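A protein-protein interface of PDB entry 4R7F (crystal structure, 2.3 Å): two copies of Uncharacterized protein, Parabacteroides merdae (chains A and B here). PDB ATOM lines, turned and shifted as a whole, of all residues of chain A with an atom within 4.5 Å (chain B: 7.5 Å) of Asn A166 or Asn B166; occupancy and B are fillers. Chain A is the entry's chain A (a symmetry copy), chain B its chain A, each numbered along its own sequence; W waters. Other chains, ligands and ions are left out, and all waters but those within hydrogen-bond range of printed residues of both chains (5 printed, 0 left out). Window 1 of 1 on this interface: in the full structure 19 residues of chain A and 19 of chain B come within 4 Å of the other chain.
The side-chain hydroxyl (OG1) of Thr B211 lies within hydrogen-bond range of the side-chain amide nitrogen (NE2) of Gln A207 (3.5 Å).
NE2 of Gln B207 lies within hydrogen-bond range of OD1 of Asn A166, 3.1 Å away.
NE2 of Gln B207 is in hydrogen-bond range of OG1 of Thr A211 (3.5 Å).
The side-chain amide oxygen (OE1) of Gln B207 lies within hydrogen-bond range of the side-chain hydroxyl (OG) of Ser A209 (3.2 Å).
The side-chain amide nitrogen of Asn A166 lies close to the side-chain amide nitrogen of Asn B166.
The side-chain hydroxyl (OG) of Ser B209 is in hydrogen-bond range of the side-chain amide oxygen (OE1) of Gln A207 (3.2 Å).
OD1 of Asn B166 is in hydrogen-bond range of NE2 of Gln A207 (3.1 Å).
The side-chain hydroxyl of Ser A145 lies within hydrogen-bond range of the side-chain hydroxyl of Ser B147, at 2.8 Å.
The side-chain hydroxyl (OG) of Ser B147 sits at hydrogen-bond distance from the side-chain amide nitrogen (ND2) of Asn A143 (2.9 Å).
Ser B147 touches Ile A144 (CB to O, 3.3 Å).
Ala B146 touches Ser A145 (O to CA, 3.7 Å).
CB of Ser B164 touches OG of Ser A145, 3.6 Å away.
Thr B211 touches Asn A168.
OD1 of Asn B168 touches CG2 of Thr A211 (3.7 Å).
Printed residues of chain A that touch a printed residue of chain B: Asn A143, Ile A144, Ser A145, Asn A166, Asn A168, Gln A207, Ser A209 and Thr A211.
Along chain A the printed residues that touch a printed residue of chain B span positions 143 to 211.
Printed residues of chain B that touch a printed residue of chain A: Ala B146, Ser B147, Ser B164, Asn B166, Asn B168, Gln B207, Ser B209 and Thr B211.
Among the printed residues, 14 pairs touch across the chains.
The backbone carbonyl oxygen (O) of Ser A145 is in hydrogen-bond range of the backbone NH (N) of Asn A166, at 2.9 Å.
The side-chain amide nitrogen (NE2) of Gln B207 sits at hydrogen-bond distance from the side-chain amide oxygen (OD1) of Asn B168, 2.8 Å away.
OD1 of Asn B166 sits at hydrogen-bond distance from OG of Ser B209.
N of Ser B147 is in hydrogen-bond range of O of Ser B164 (2.9 Å).
OG of Ser A209 is in hydrogen-bond range of OG1 of Thr A211.
OG of Ser A145 sits at hydrogen-bond distance from ND2 of Asn A168, 3.0 Å away.
Asn B166 touches its own counterpart, Asn A166.
Asn A166 touches Gln B207, and with the chains exchanged Gln A207 touches Asn B166.
Asn A168 touches Thr B211, and with the chains exchanged Thr A211 touches Asn B168.
Gln A207 touches Ser B209, and with the chains exchanged Ser A209 touches Gln B207.
Of the 14 pairs that touch across the chains among the printed residues, 9 have their exchanged pair printed and touching as well.
Of the printed residues of chain B, Ser A145 touches Ala B146, Ser B147 and Ser B164.
Of the printed residues of chain B, Asn A166 touches Asn B166 and Gln B207.
Val B142 touches none of the printed residues of chain A.
Printed residues of chain A within 4 Å of Ala B146: Ser A145 (3.7 Å).
Printed residues of chain A within 4 Å of Ser B147: Asn A143, Ile A144 and Ser A145.
Printed residues of chain A within 4 Å of Asn B166: Asn A166 and Gln A207.
Printed residues of chain A within 4 Å of Ser B209: Gln A207 (3.2 Å).
Of the printed residues of chain A, Thr B211 touches Asn A168 (3.7 Å) and Gln A207 (3.5 Å).
Val B378 touches none of the printed residues of chain A.
The nearest printed residue of chain B that does not touch Asn A166 is Ser B145 (4.1 Å).
Water W3 lies within hydrogen-bond range of the side-chain amide nitrogen (ND2) of Asn A166 (2.7 Å), the side-chain hydroxyl (OG1) of Thr A211 (2.7 Å), the side-chain hydroxyl (OG) of Ser B145 (3.0 Å) and the side-chain amide nitrogen (ND2) of Asn B168 (3.4 Å).
Water W4 lies within hydrogen-bond range of ND2 of Asn B166 (2.7 Å), OG1 of Thr B211 (2.7 Å), OG of Ser A145 (3.0 Å) and ND2 of Asn A168 (3.4 Å).
Water W2 lies within hydrogen-bond range of OG of Ser B164 (2.7 Å), ND2 of Asn A143 (3.2 Å) and OG of Ser B147 (3.4 Å).
Water W1 lies within hydrogen-bond range of the side-chain amide oxygen (OD1) of Asn A143 and the side-chain hydroxyl (OG) of Ser B164.
Water W5 bridges O of Ala B146 (3.0 Å) and O of Ile A144 (3.5 Å).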
ATOM      1  N   ASN A 143      36.089 -11.277  -5.677  1.00  0.00           N
ATOM      2  CA  ASN A 143      35.467 -10.472  -4.630  1.00  0.00           C
ATOM      3  C   ASN A 143      34.092 -11.100  -4.398  1.00  0.00           C
ATOM      4  O   ASN A 143      33.459 -11.577  -5.350  1.00  0.00           O
ATOM      5  CB  ASN A 143      35.451  -8.977  -5.089  1.00  0.00           C
ATOM      6  CG  ASN A 143      34.306  -8.159  -4.521  1.00  0.00           C
ATOM      7  OD1 ASN A 143      33.213  -8.159  -5.081  1.00  0.00           O
ATOM      8  ND2 ASN A 143      34.559  -7.413  -3.445  1.00  0.00           N
ATOM      9  N   ILE A 144      33.632 -11.143  -3.153  1.00  0.00           N
ATOM     10  CA  ILE A 144      32.340 -11.721  -2.846  1.00  0.00           C
ATOM     11  C   ILE A 144      31.461 -10.661  -2.226  1.00  0.00           C
ATOM     12  O   ILE A 144      31.814 -10.108  -1.181  1.00  0.00           O
ATOM     13  CB  ILE A 144      32.491 -12.895  -1.866  1.00  0.00           C
ATOM     14  CG1 ILE A 144      33.402 -13.994  -2.431  1.00  0.00           C
ATOM     15  CG2 ILE A 144      31.125 -13.476  -1.536  1.00  0.00           C
ATOM     16  CD1 ILE A 144      33.742 -15.096  -1.418  1.00  0.00           C
ATOM     17  N   SER A 145      30.340 -10.345  -2.872  1.00  0.00           N
ATOM     18  CA  SER A 145      29.324  -9.443  -2.311  1.00  0.00           C
ATOM     19  C   SER A 145      28.229 -10.283  -1.690  1.00  0.00           C
ATOM     20  O   SER A 145      27.676 -11.119  -2.372  1.00  0.00           O
ATOM     21  CB  SER A 145      28.718  -8.552  -3.397  1.00  0.00           C
ATOM     22  OG  SER A 145      29.693  -7.701  -3.953  1.00  0.00           O
ATOM     23  N   PHE A 165      24.741 -14.397  -1.947  1.00  0.00           N
ATOM     24  CA  PHE A 165      26.022 -13.846  -2.397  1.00  0.00           C
ATOM     25  C   PHE A 165      26.287 -13.956  -3.881  1.00  0.00           C
ATOM     26  O   PHE A 165      25.697 -14.783  -4.547  1.00  0.00           O
ATOM     27  CB  PHE A 165      27.203 -14.408  -1.585  1.00  0.00           C
ATOM     28  CG  PHE A 165      27.560 -15.835  -1.906  1.00  0.00           C
ATOM     29  CD1 PHE A 165      26.928 -16.888  -1.259  1.00  0.00           C
ATOM     30  CD2 PHE A 165      28.548 -16.121  -2.821  1.00  0.00           C
ATOM     31  CE1 PHE A 165      27.282 -18.206  -1.541  1.00  0.00           C
ATOM     32  CE2 PHE A 165      28.877 -17.431  -3.136  1.00  0.00           C
ATOM     33  CZ  PHE A 165      28.255 -18.470  -2.479  1.00  0.00           C
ATOM     34  N   ASN A 166      27.214 -13.125  -4.361  1.00  0.00           N
ATOM     35  CA  ASN A 166      27.656 -13.124  -5.767  1.00  0.00           C
ATOM     36  C   ASN A 166      29.139 -13.136  -5.764  1.00  0.00           C
ATOM     37  O   ASN A 166      29.756 -12.464  -4.954  1.00  0.00           O
ATOM     38  CB  ASN A 166      27.201 -11.872  -6.518  1.00  0.00           C
ATOM     39  CG  ASN A 166      25.702 -11.671  -6.426  1.00  0.00           C
ATOM     40  OD1 ASN A 166      24.948 -12.230  -7.205  1.00  0.00           O
ATOM     41  ND2 ASN A 166      25.268 -10.896  -5.430  1.00  0.00           N
ATOM     42  N   ILE A 167      29.705 -13.895  -6.685  1.00  0.00           N
ATOM     43  CA  ILE A 167      31.112 -13.914  -6.871  1.00  0.00           C
ATOM     44  C   ILE A 167      31.378 -13.016  -8.047  1.00  0.00           C
ATOM     45  O   ILE A 167      30.896 -13.279  -9.128  1.00  0.00           O
ATOM     46  CB  ILE A 167      31.608 -15.330  -7.195  1.00  0.00           C
ATOM     47  CG1 ILE A 167      31.275 -16.258  -6.030  1.00  0.00           C
ATOM     48  CG2 ILE A 167      33.097 -15.300  -7.482  1.00  0.00           C
ATOM     49  CD1 ILE A 167      31.593 -17.705  -6.314  1.00  0.00           C
ATOM     50  N   ASN A 168      32.125 -11.948  -7.797  1.00  0.00           N
ATOM     51  CA  ASN A 168      32.552 -11.002  -8.800  1.00  0.00           C
ATOM     52  C   ASN A 168      33.955 -11.329  -9.314  1.00  0.00           C
ATOM     53  O   ASN A 168      34.915 -11.147  -8.608  1.00  0.00           O
ATOM     54  CB  ASN A 168      32.495  -9.604  -8.184  1.00  0.00           C
ATOM     55  CG  ASN A 168      31.108  -9.270  -7.620  1.00  0.00           C
ATOM     56  OD1 ASN A 168      30.084  -9.544  -8.241  1.00  0.00           O
ATOM     57  ND2 ASN A 168      31.085  -8.673  -6.447  1.00  0.00           N
ATOM     58  N   GLN A 207      30.128 -12.510 -13.258  1.00  0.00           N
ATOM     59  CA  GLN A 207      29.361 -12.570 -12.023  1.00  0.00           C
ATOM     60  C   GLN A 207      28.622 -13.849 -11.903  1.00  0.00           C
ATOM     61  O   GLN A 207      27.938 -14.231 -12.823  1.00  0.00           O
ATOM     62  CB  GLN A 207      28.353 -11.445 -11.925  1.00  0.00           C
ATOM     63  CG  GLN A 207      27.878 -11.322 -10.506  1.00  0.00           C
ATOM     64  CD  GLN A 207      27.051 -10.072 -10.267  1.00  0.00           C
ATOM     65  OE1 GLN A 207      25.999  -9.879 -10.911  1.00  0.00           O
ATOM     66  NE2 GLN A 207      27.494  -9.231  -9.313  1.00  0.00           N
ATOM     67  N   ILE A 208      28.802 -14.512 -10.770  1.00  0.00           N
ATOM     68  CA  ILE A 208      28.150 -15.770 -10.485  1.00  0.00           C
ATOM     69  C   ILE A 208      27.300 -15.568  -9.255  1.00  0.00           C
ATOM     70  O   ILE A 208      27.812 -15.241  -8.195  1.00  0.00           O
ATOM     71  CB  ILE A 208      29.165 -16.890 -10.235  1.00  0.00           C
ATOM     72  CG1 ILE A 208      30.193 -16.937 -11.375  1.00  0.00           C
ATOM     73  CG2 ILE A 208      28.454 -18.253 -10.154  1.00  0.00           C
ATOM     74  CD1 ILE A 208      31.607 -17.210 -10.911  1.00  0.00           C
ATOM     75  N   SER A 209      25.999 -15.759  -9.395  1.00  0.00           N
ATOM     76  CA  SER A 209      25.079 -15.442  -8.309  1.00  0.00           C
ATOM     77  C   SER A 209      24.553 -16.702  -7.634  1.00  0.00           C
ATOM     78  O   SER A 209      24.103 -17.627  -8.329  1.00  0.00           O
ATOM     79  CB  SER A 209      23.927 -14.576  -8.845  1.00  0.00           C
ATOM     80  OG  SER A 209      22.932 -14.382  -7.848  1.00  0.00           O
ATOM     81  N   THR A 211      22.051 -16.776  -5.157  1.00  0.00           N
ATOM     82  CA  THR A 211      21.034 -16.034  -4.456  1.00  0.00           C
ATOM     83  C   THR A 211      19.762 -16.827  -4.605  1.00  0.00           C
ATOM     84  O   THR A 211      19.563 -17.427  -5.630  1.00  0.00           O
ATOM     85  CB  THR A 211      20.894 -14.642  -5.082  1.00  0.00           C
ATOM     86  OG1 THR A 211      22.138 -13.955  -4.922  1.00  0.00           O
ATOM     87  CG2 THR A 211      19.856 -13.848  -4.379  1.00  0.00           C
ATOM     88  N   VAL B 142      13.128  -5.057  -1.027  1.00  0.00           N
ATOM     89  CA  VAL B 142      14.209  -5.697  -1.715  1.00  0.00           C
ATOM     90  C   VAL B 142      15.391  -5.850  -0.734  1.00  0.00           C
ATOM     91  O   VAL B 142      15.484  -5.141   0.265  1.00  0.00           O
ATOM     92  CB  VAL B 142      14.633  -4.905  -2.965  1.00  0.00           C
ATOM     93  CG1 VAL B 142      13.453  -4.667  -3.886  1.00  0.00           C
ATOM     94  CG2 VAL B 142      15.280  -3.582  -2.577  1.00  0.00           C
ATOM     95  N   ASN B 143      16.276  -6.784  -1.035  1.00  0.00           N
ATOM     96  CA  ASN B 143      17.442  -7.112  -0.220  1.00  0.00           C
ATOM     97  C   ASN B 143      18.649  -6.631  -1.027  1.00  0.00           C
ATOM     98  O   ASN B 143      18.642  -6.715  -2.263  1.00  0.00           O
ATOM     99  CB  ASN B 143      17.416  -8.643   0.098  1.00  0.00           C
ATOM    100  CG  ASN B 143      18.787  -9.264   0.298  1.00  0.00           C
ATOM    101  OD1 ASN B 143      19.433  -9.656  -0.669  1.00  0.00           O
ATOM    102  ND2 ASN B 143      19.214  -9.414   1.553  1.00  0.00           N
ATOM    103  N   ILE B 144      19.668  -6.099  -0.362  1.00  0.00           N
ATOM    104  CA  ILE B 144      20.848  -5.619  -1.049  1.00  0.00           C
ATOM    105  C   ILE B 144      22.050  -6.396  -0.566  1.00  0.00           C
ATOM    106  O   ILE B 144      22.351  -6.376   0.630  1.00  0.00           O
ATOM    107  CB  ILE B 144      21.065  -4.123  -0.771  1.00  0.00           C
ATOM    108  CG1 ILE B 144      19.859  -3.282  -1.214  1.00  0.00           C
ATOM    109  CG2 ILE B 144      22.320  -3.638  -1.481  1.00  0.00           C
ATOM    110  CD1 ILE B 144      19.941  -1.811  -0.785  1.00  0.00           C
ATOM    111  N   SER B 145      22.717  -7.110  -1.471  1.00  0.00           N
ATOM    112  CA  SER B 145      23.984  -7.791  -1.173  1.00  0.00           C
ATOM    113  C   SER B 145      25.123  -6.913  -1.645  1.00  0.00           C
ATOM    114  O   SER B 145      25.139  -6.548  -2.801  1.00  0.00           O
ATOM    115  CB  SER B 145      24.065  -9.143  -1.886  1.00  0.00           C
ATOM    116  OG  SER B 145      23.062 -10.017  -1.422  1.00  0.00           O
ATOM    117  N   ALA B 146      26.067  -6.601  -0.752  1.00  0.00           N
ATOM    118  CA  ALA B 146      27.105  -5.612  -1.040  1.00  0.00           C
ATOM    119  C   ALA B 146      28.488  -6.029  -0.547  1.00  0.00           C
ATOM    120  O   ALA B 146      28.615  -6.902   0.287  1.00  0.00           O
ATOM    121  CB  ALA B 146      26.719  -4.261  -0.453  1.00  0.00           C
ATOM    122  N   SER B 147      29.526  -5.440  -1.138  1.00  0.00           N
ATOM    123  CA  SER B 147      30.876  -5.591  -0.622  1.00  0.00           C
ATOM    124  C   SER B 147      31.674  -4.300  -0.837  1.00  0.00           C
ATOM    125  O   SER B 147      31.320  -3.506  -1.684  1.00  0.00           O
ATOM    126  CB  SER B 147      31.594  -6.781  -1.274  1.00  0.00           C
ATOM    127  OG  SER B 147      31.870  -6.542  -2.645  1.00  0.00           O
ATOM    128  N   SER B 164      30.394  -2.527  -4.335  1.00  0.00           N
ATOM    129  CA  SER B 164      29.822  -3.416  -5.340  1.00  0.00           C
ATOM    130  C   SER B 164      28.529  -3.851  -4.692  1.00  0.00           C
ATOM    131  O   SER B 164      28.520  -4.165  -3.496  1.00  0.00           O
ATOM    132  CB  SER B 164      30.729  -4.641  -5.583  1.00  0.00           C
ATOM    133  OG  SER B 164      32.064  -4.326  -6.006  1.00  0.00           O
ATOM    134  N   PHE B 165      27.427  -3.836  -5.436  1.00  0.00           N
ATOM    135  CA  PHE B 165      26.180  -4.357  -4.872  1.00  0.00           C
ATOM    136  C   PHE B 165      25.186  -4.885  -5.881  1.00  0.00           C
ATOM    137  O   PHE B 165      25.242  -4.526  -7.040  1.00  0.00           O
ATOM    138  CB  PHE B 165      25.514  -3.345  -3.924  1.00  0.00           C
ATOM    139  CG  PHE B 165      24.861  -2.176  -4.613  1.00  0.00           C
ATOM    140  CD1 PHE B 165      25.590  -1.037  -4.926  1.00  0.00           C
ATOM    141  CD2 PHE B 165      23.518  -2.202  -4.914  1.00  0.00           C
ATOM    142  CE1 PHE B 165      24.975   0.051  -5.541  1.00  0.00           C
ATOM    143  CE2 PHE B 165      22.907  -1.138  -5.562  1.00  0.00           C
ATOM    144  CZ  PHE B 165      23.636  -0.006  -5.855  1.00  0.00           C
ATOM    145  N   ASN B 166      24.261  -5.715  -5.395  1.00  0.00           N
ATOM    146  CA  ASN B 166      23.171  -6.284  -6.208  1.00  0.00           C
ATOM    147  C   ASN B 166      21.908  -6.079  -5.456  1.00  0.00           C
ATOM    148  O   ASN B 166      21.881  -6.234  -4.247  1.00  0.00           O
ATOM    149  CB  ASN B 166      23.340  -7.786  -6.435  1.00  0.00           C
ATOM    150  CG  ASN B 166      24.689  -8.119  -7.039  1.00  0.00           C
ATOM    151  OD1 ASN B 166      24.863  -8.068  -8.246  1.00  0.00           O
ATOM    152  ND2 ASN B 166      25.665  -8.419  -6.180  1.00  0.00           N
ATOM    153  N   ILE B 167      20.859  -5.743  -6.186  1.00  0.00           N
ATOM    154  CA  ILE B 167      19.564  -5.626  -5.617  1.00  0.00           C
ATOM    155  C   ILE B 167      18.857  -6.910  -5.950  1.00  0.00           C
ATOM    156  O   ILE B 167      18.684  -7.220  -7.109  1.00  0.00           O
ATOM    157  CB  ILE B 167      18.793  -4.451  -6.234  1.00  0.00           C
ATOM    158  CG1 ILE B 167      19.548  -3.153  -5.957  1.00  0.00           C
ATOM    159  CG2 ILE B 167      17.383  -4.411  -5.676  1.00  0.00           C
ATOM    160  CD1 ILE B 167      18.945  -1.956  -6.649  1.00  0.00           C
ATOM    161  N   ASN B 168      18.487  -7.648  -4.911  1.00  0.00           N
ATOM    162  CA  ASN B 168      17.737  -8.877  -5.013  1.00  0.00           C
ATOM    163  C   ASN B 168      16.238  -8.633  -4.825  1.00  0.00           C
ATOM    164  O   ASN B 168      15.803  -8.356  -3.736  1.00  0.00           O
ATOM    165  CB  ASN B 168      18.280  -9.849  -3.965  1.00  0.00           C
ATOM    166  CG  ASN B 168      19.791 -10.074  -4.106  1.00  0.00           C
ATOM    167  OD1 ASN B 168      20.312 -10.241  -5.206  1.00  0.00           O
ATOM    168  ND2 ASN B 168      20.484 -10.084  -2.987  1.00  0.00           N
ATOM    169  N   ASN B 169      15.471  -8.747  -5.919  1.00  0.00           N
ATOM    170  CA  ASN B 169      14.085  -8.342  -5.979  1.00  0.00           C
ATOM    171  C   ASN B 169      13.114  -9.397  -6.500  1.00  0.00           C
ATOM    172  O   ASN B 169      12.124  -9.043  -7.131  1.00  0.00           O
ATOM    173  CB  ASN B 169      13.920  -7.046  -6.819  1.00  0.00           C
ATOM    174  CG  ASN B 169      14.208  -7.255  -8.299  1.00  0.00           C
ATOM    175  OD1 ASN B 169      15.022  -8.081  -8.687  1.00  0.00           O
ATOM    176  ND2 ASN B 169      13.503  -6.543  -9.120  1.00  0.00           N
ATOM    177  N   SER B 202      24.051  -5.020 -15.125  1.00  0.00           N
ATOM    178  CA  SER B 202      23.199  -6.111 -15.667  1.00  0.00           C
ATOM    179  C   SER B 202      21.850  -6.201 -14.973  1.00  0.00           C
ATOM    180  O   SER B 202      21.752  -5.881 -13.802  1.00  0.00           O
ATOM    181  CB  SER B 202      23.897  -7.471 -15.511  1.00  0.00           C
ATOM    182  OG  SER B 202      23.984  -7.824 -14.134  1.00  0.00           O
ATOM    183  N   ASN B 206      15.232 -11.061 -11.465  1.00  0.00           N
ATOM    184  CA  ASN B 206      15.226 -11.044 -10.009  1.00  0.00           C
ATOM    185  C   ASN B 206      16.558 -10.552  -9.403  1.00  0.00           C
ATOM    186  O   ASN B 206      16.864 -10.808  -8.216  1.00  0.00           O
ATOM    187  CB  ASN B 206      14.882 -12.436  -9.469  1.00  0.00           C
ATOM    188  CG  ASN B 206      15.789 -13.534 -10.019  1.00  0.00           C
ATOM    189  OD1 ASN B 206      16.928 -13.263 -10.436  1.00  0.00           O
ATOM    190  ND2 ASN B 206      15.289 -14.804 -10.010  1.00  0.00           N
ATOM    191  N   GLN B 207      17.340  -9.839 -10.203  1.00  0.00           N
ATOM    192  CA  GLN B 207      18.613  -9.336  -9.709  1.00  0.00           C
ATOM    193  C   GLN B 207      19.137  -8.246 -10.565  1.00  0.00           C
ATOM    194  O   GLN B 207      19.203  -8.405 -11.761  1.00  0.00           O
ATOM    195  CB  GLN B 207      19.667 -10.420  -9.649  1.00  0.00           C
ATOM    196  CG  GLN B 207      20.808  -9.960  -8.788  1.00  0.00           C
ATOM    197  CD  GLN B 207      21.796 -11.069  -8.475  1.00  0.00           C
ATOM    198  OE1 GLN B 207      22.390 -11.663  -9.399  1.00  0.00           O
ATOM    199  NE2 GLN B 207      22.013 -11.332  -7.173  1.00  0.00           N
ATOM    200  N   ILE B 208      19.473  -7.131  -9.932  1.00  0.00           N
ATOM    201  CA  ILE B 208      20.009  -5.973 -10.613  1.00  0.00           C
ATOM    202  C   ILE B 208      21.385  -5.716 -10.048  1.00  0.00           C
ATOM    203  O   ILE B 208      21.529  -5.468  -8.861  1.00  0.00           O
ATOM    204  CB  ILE B 208      19.126  -4.738 -10.411  1.00  0.00           C
ATOM    205  CG1 ILE B 208      17.666  -5.070 -10.751  1.00  0.00           C
ATOM    206  CG2 ILE B 208      19.596  -3.587 -11.319  1.00  0.00           C
ATOM    207  CD1 ILE B 208      16.662  -4.437  -9.812  1.00  0.00           C
ATOM    208  N   SER B 209      22.396  -5.778 -10.897  1.00  0.00           N
ATOM    209  CA  SER B 209      23.773  -5.696 -10.422  1.00  0.00           C
ATOM    210  C   SER B 209      24.399  -4.347 -10.752  1.00  0.00           C
ATOM    211  O   SER B 209      24.309  -3.895 -11.905  1.00  0.00           O
ATOM    212  CB  SER B 209      24.593  -6.851 -11.018  1.00  0.00           C
ATOM    213  OG  SER B 209      25.972  -6.709 -10.702  1.00  0.00           O
ATOM    214  N   TYR B 210      24.991  -3.700  -9.737  1.00  0.00           N
ATOM    215  CA  TYR B 210      25.706  -2.416  -9.914  1.00  0.00           C
ATOM    216  C   TYR B 210      27.123  -2.662  -9.485  1.00  0.00           C
ATOM    217  O   TYR B 210      27.591  -2.162  -8.478  1.00  0.00           O
ATOM    218  CB  TYR B 210      25.128  -1.285  -9.048  1.00  0.00           C
ATOM    219  CG  TYR B 210      23.716  -0.927  -9.368  1.00  0.00           C
ATOM    220  CD1 TYR B 210      22.667  -1.696  -8.906  1.00  0.00           C
ATOM    221  CD2 TYR B 210      23.419   0.160 -10.175  1.00  0.00           C
ATOM    222  CE1 TYR B 210      21.350  -1.391  -9.230  1.00  0.00           C
ATOM    223  CE2 TYR B 210      22.103   0.493 -10.472  1.00  0.00           C
ATOM    224  CZ  TYR B 210      21.068  -0.287 -10.006  1.00  0.00           C
ATOM    225  OH  TYR B 210      19.748   0.033 -10.309  1.00  0.00           O
ATOM    226  N   THR B 211      27.778  -3.505 -10.229  1.00  0.00           N
ATOM    227  CA  THR B 211      29.097  -3.983  -9.898  1.00  0.00           C
ATOM    228  C   THR B 211      30.001  -3.512 -11.007  1.00  0.00           C
ATOM    229  O   THR B 211      29.572  -3.463 -12.131  1.00  0.00           O
ATOM    230  CB  THR B 211      29.079  -5.513  -9.812  1.00  0.00           C
ATOM    231  OG1 THR B 211      28.191  -5.890  -8.756  1.00  0.00           O
ATOM    232  CG2 THR B 211      30.423  -6.039  -9.468  1.00  0.00           C
ATOM    233  N   ILE B 376      23.751   2.413   1.151  1.00  0.00           N
ATOM    234  CA  ILE B 376      23.181   2.289  -0.184  1.00  0.00           C
ATOM    235  C   ILE B 376      21.676   2.392  -0.024  1.00  0.00           C
ATOM    236  O   ILE B 376      21.066   1.592   0.676  1.00  0.00           O
ATOM    237  CB  ILE B 376      23.534   0.944  -0.787  1.00  0.00           C
ATOM    238  CG1 ILE B 376      25.058   0.808  -0.838  1.00  0.00           C
ATOM    239  CG2 ILE B 376      22.943   0.785  -2.190  1.00  0.00           C
ATOM    240  CD1 ILE B 376      25.501  -0.617  -0.992  1.00  0.00           C
ATOM    241  N   VAL B 378      18.065   2.751  -1.980  1.00  0.00           N
ATOM    242  CA  VAL B 378      17.427   2.400  -3.209  1.00  0.00           C
ATOM    243  C   VAL B 378      16.007   2.967  -3.198  1.00  0.00           C
ATOM    244  O   VAL B 378      15.186   2.505  -2.449  1.00  0.00           O
ATOM    245  CB  VAL B 378      17.366   0.870  -3.355  1.00  0.00           C
ATOM    246  CG1 VAL B 378      16.614   0.497  -4.627  1.00  0.00           C
ATOM    247  CG2 VAL B 378      18.766   0.270  -3.360  1.00  0.00           C
ATOM    248  N   THR B 394      20.843  -0.335   2.973  1.00  0.00           N
ATOM    249  CA  THR B 394      21.780  -1.160   3.720  1.00  0.00           C
ATOM    250  C   THR B 394      23.061  -0.367   3.970  1.00  0.00           C
ATOM    251  O   THR B 394      23.374   0.548   3.231  1.00  0.00           O
ATOM    252  CB  THR B 394      22.111  -2.468   2.989  1.00  0.00           C
ATOM    253  OG1 THR B 394      22.763  -3.346   3.895  1.00  0.00           O
ATOM    254  CG2 THR B 394      23.060  -2.261   1.811  1.00  0.00           C
HETATM  255  O   HOH W   1      34.081  -6.209  -6.896  1.00  0.00           O
HETATM  256  O   HOH W   2      33.999  -4.372  -4.136  1.00  0.00           O
HETATM  257  O   HOH W   3      23.309 -11.773  -3.856  1.00  0.00           O
HETATM  258  O   HOH W   4      28.019  -7.196  -6.405  1.00  0.00           O
HETATM  259  O   HOH W   5      30.478  -8.727   1.715  1.00  0.00           O
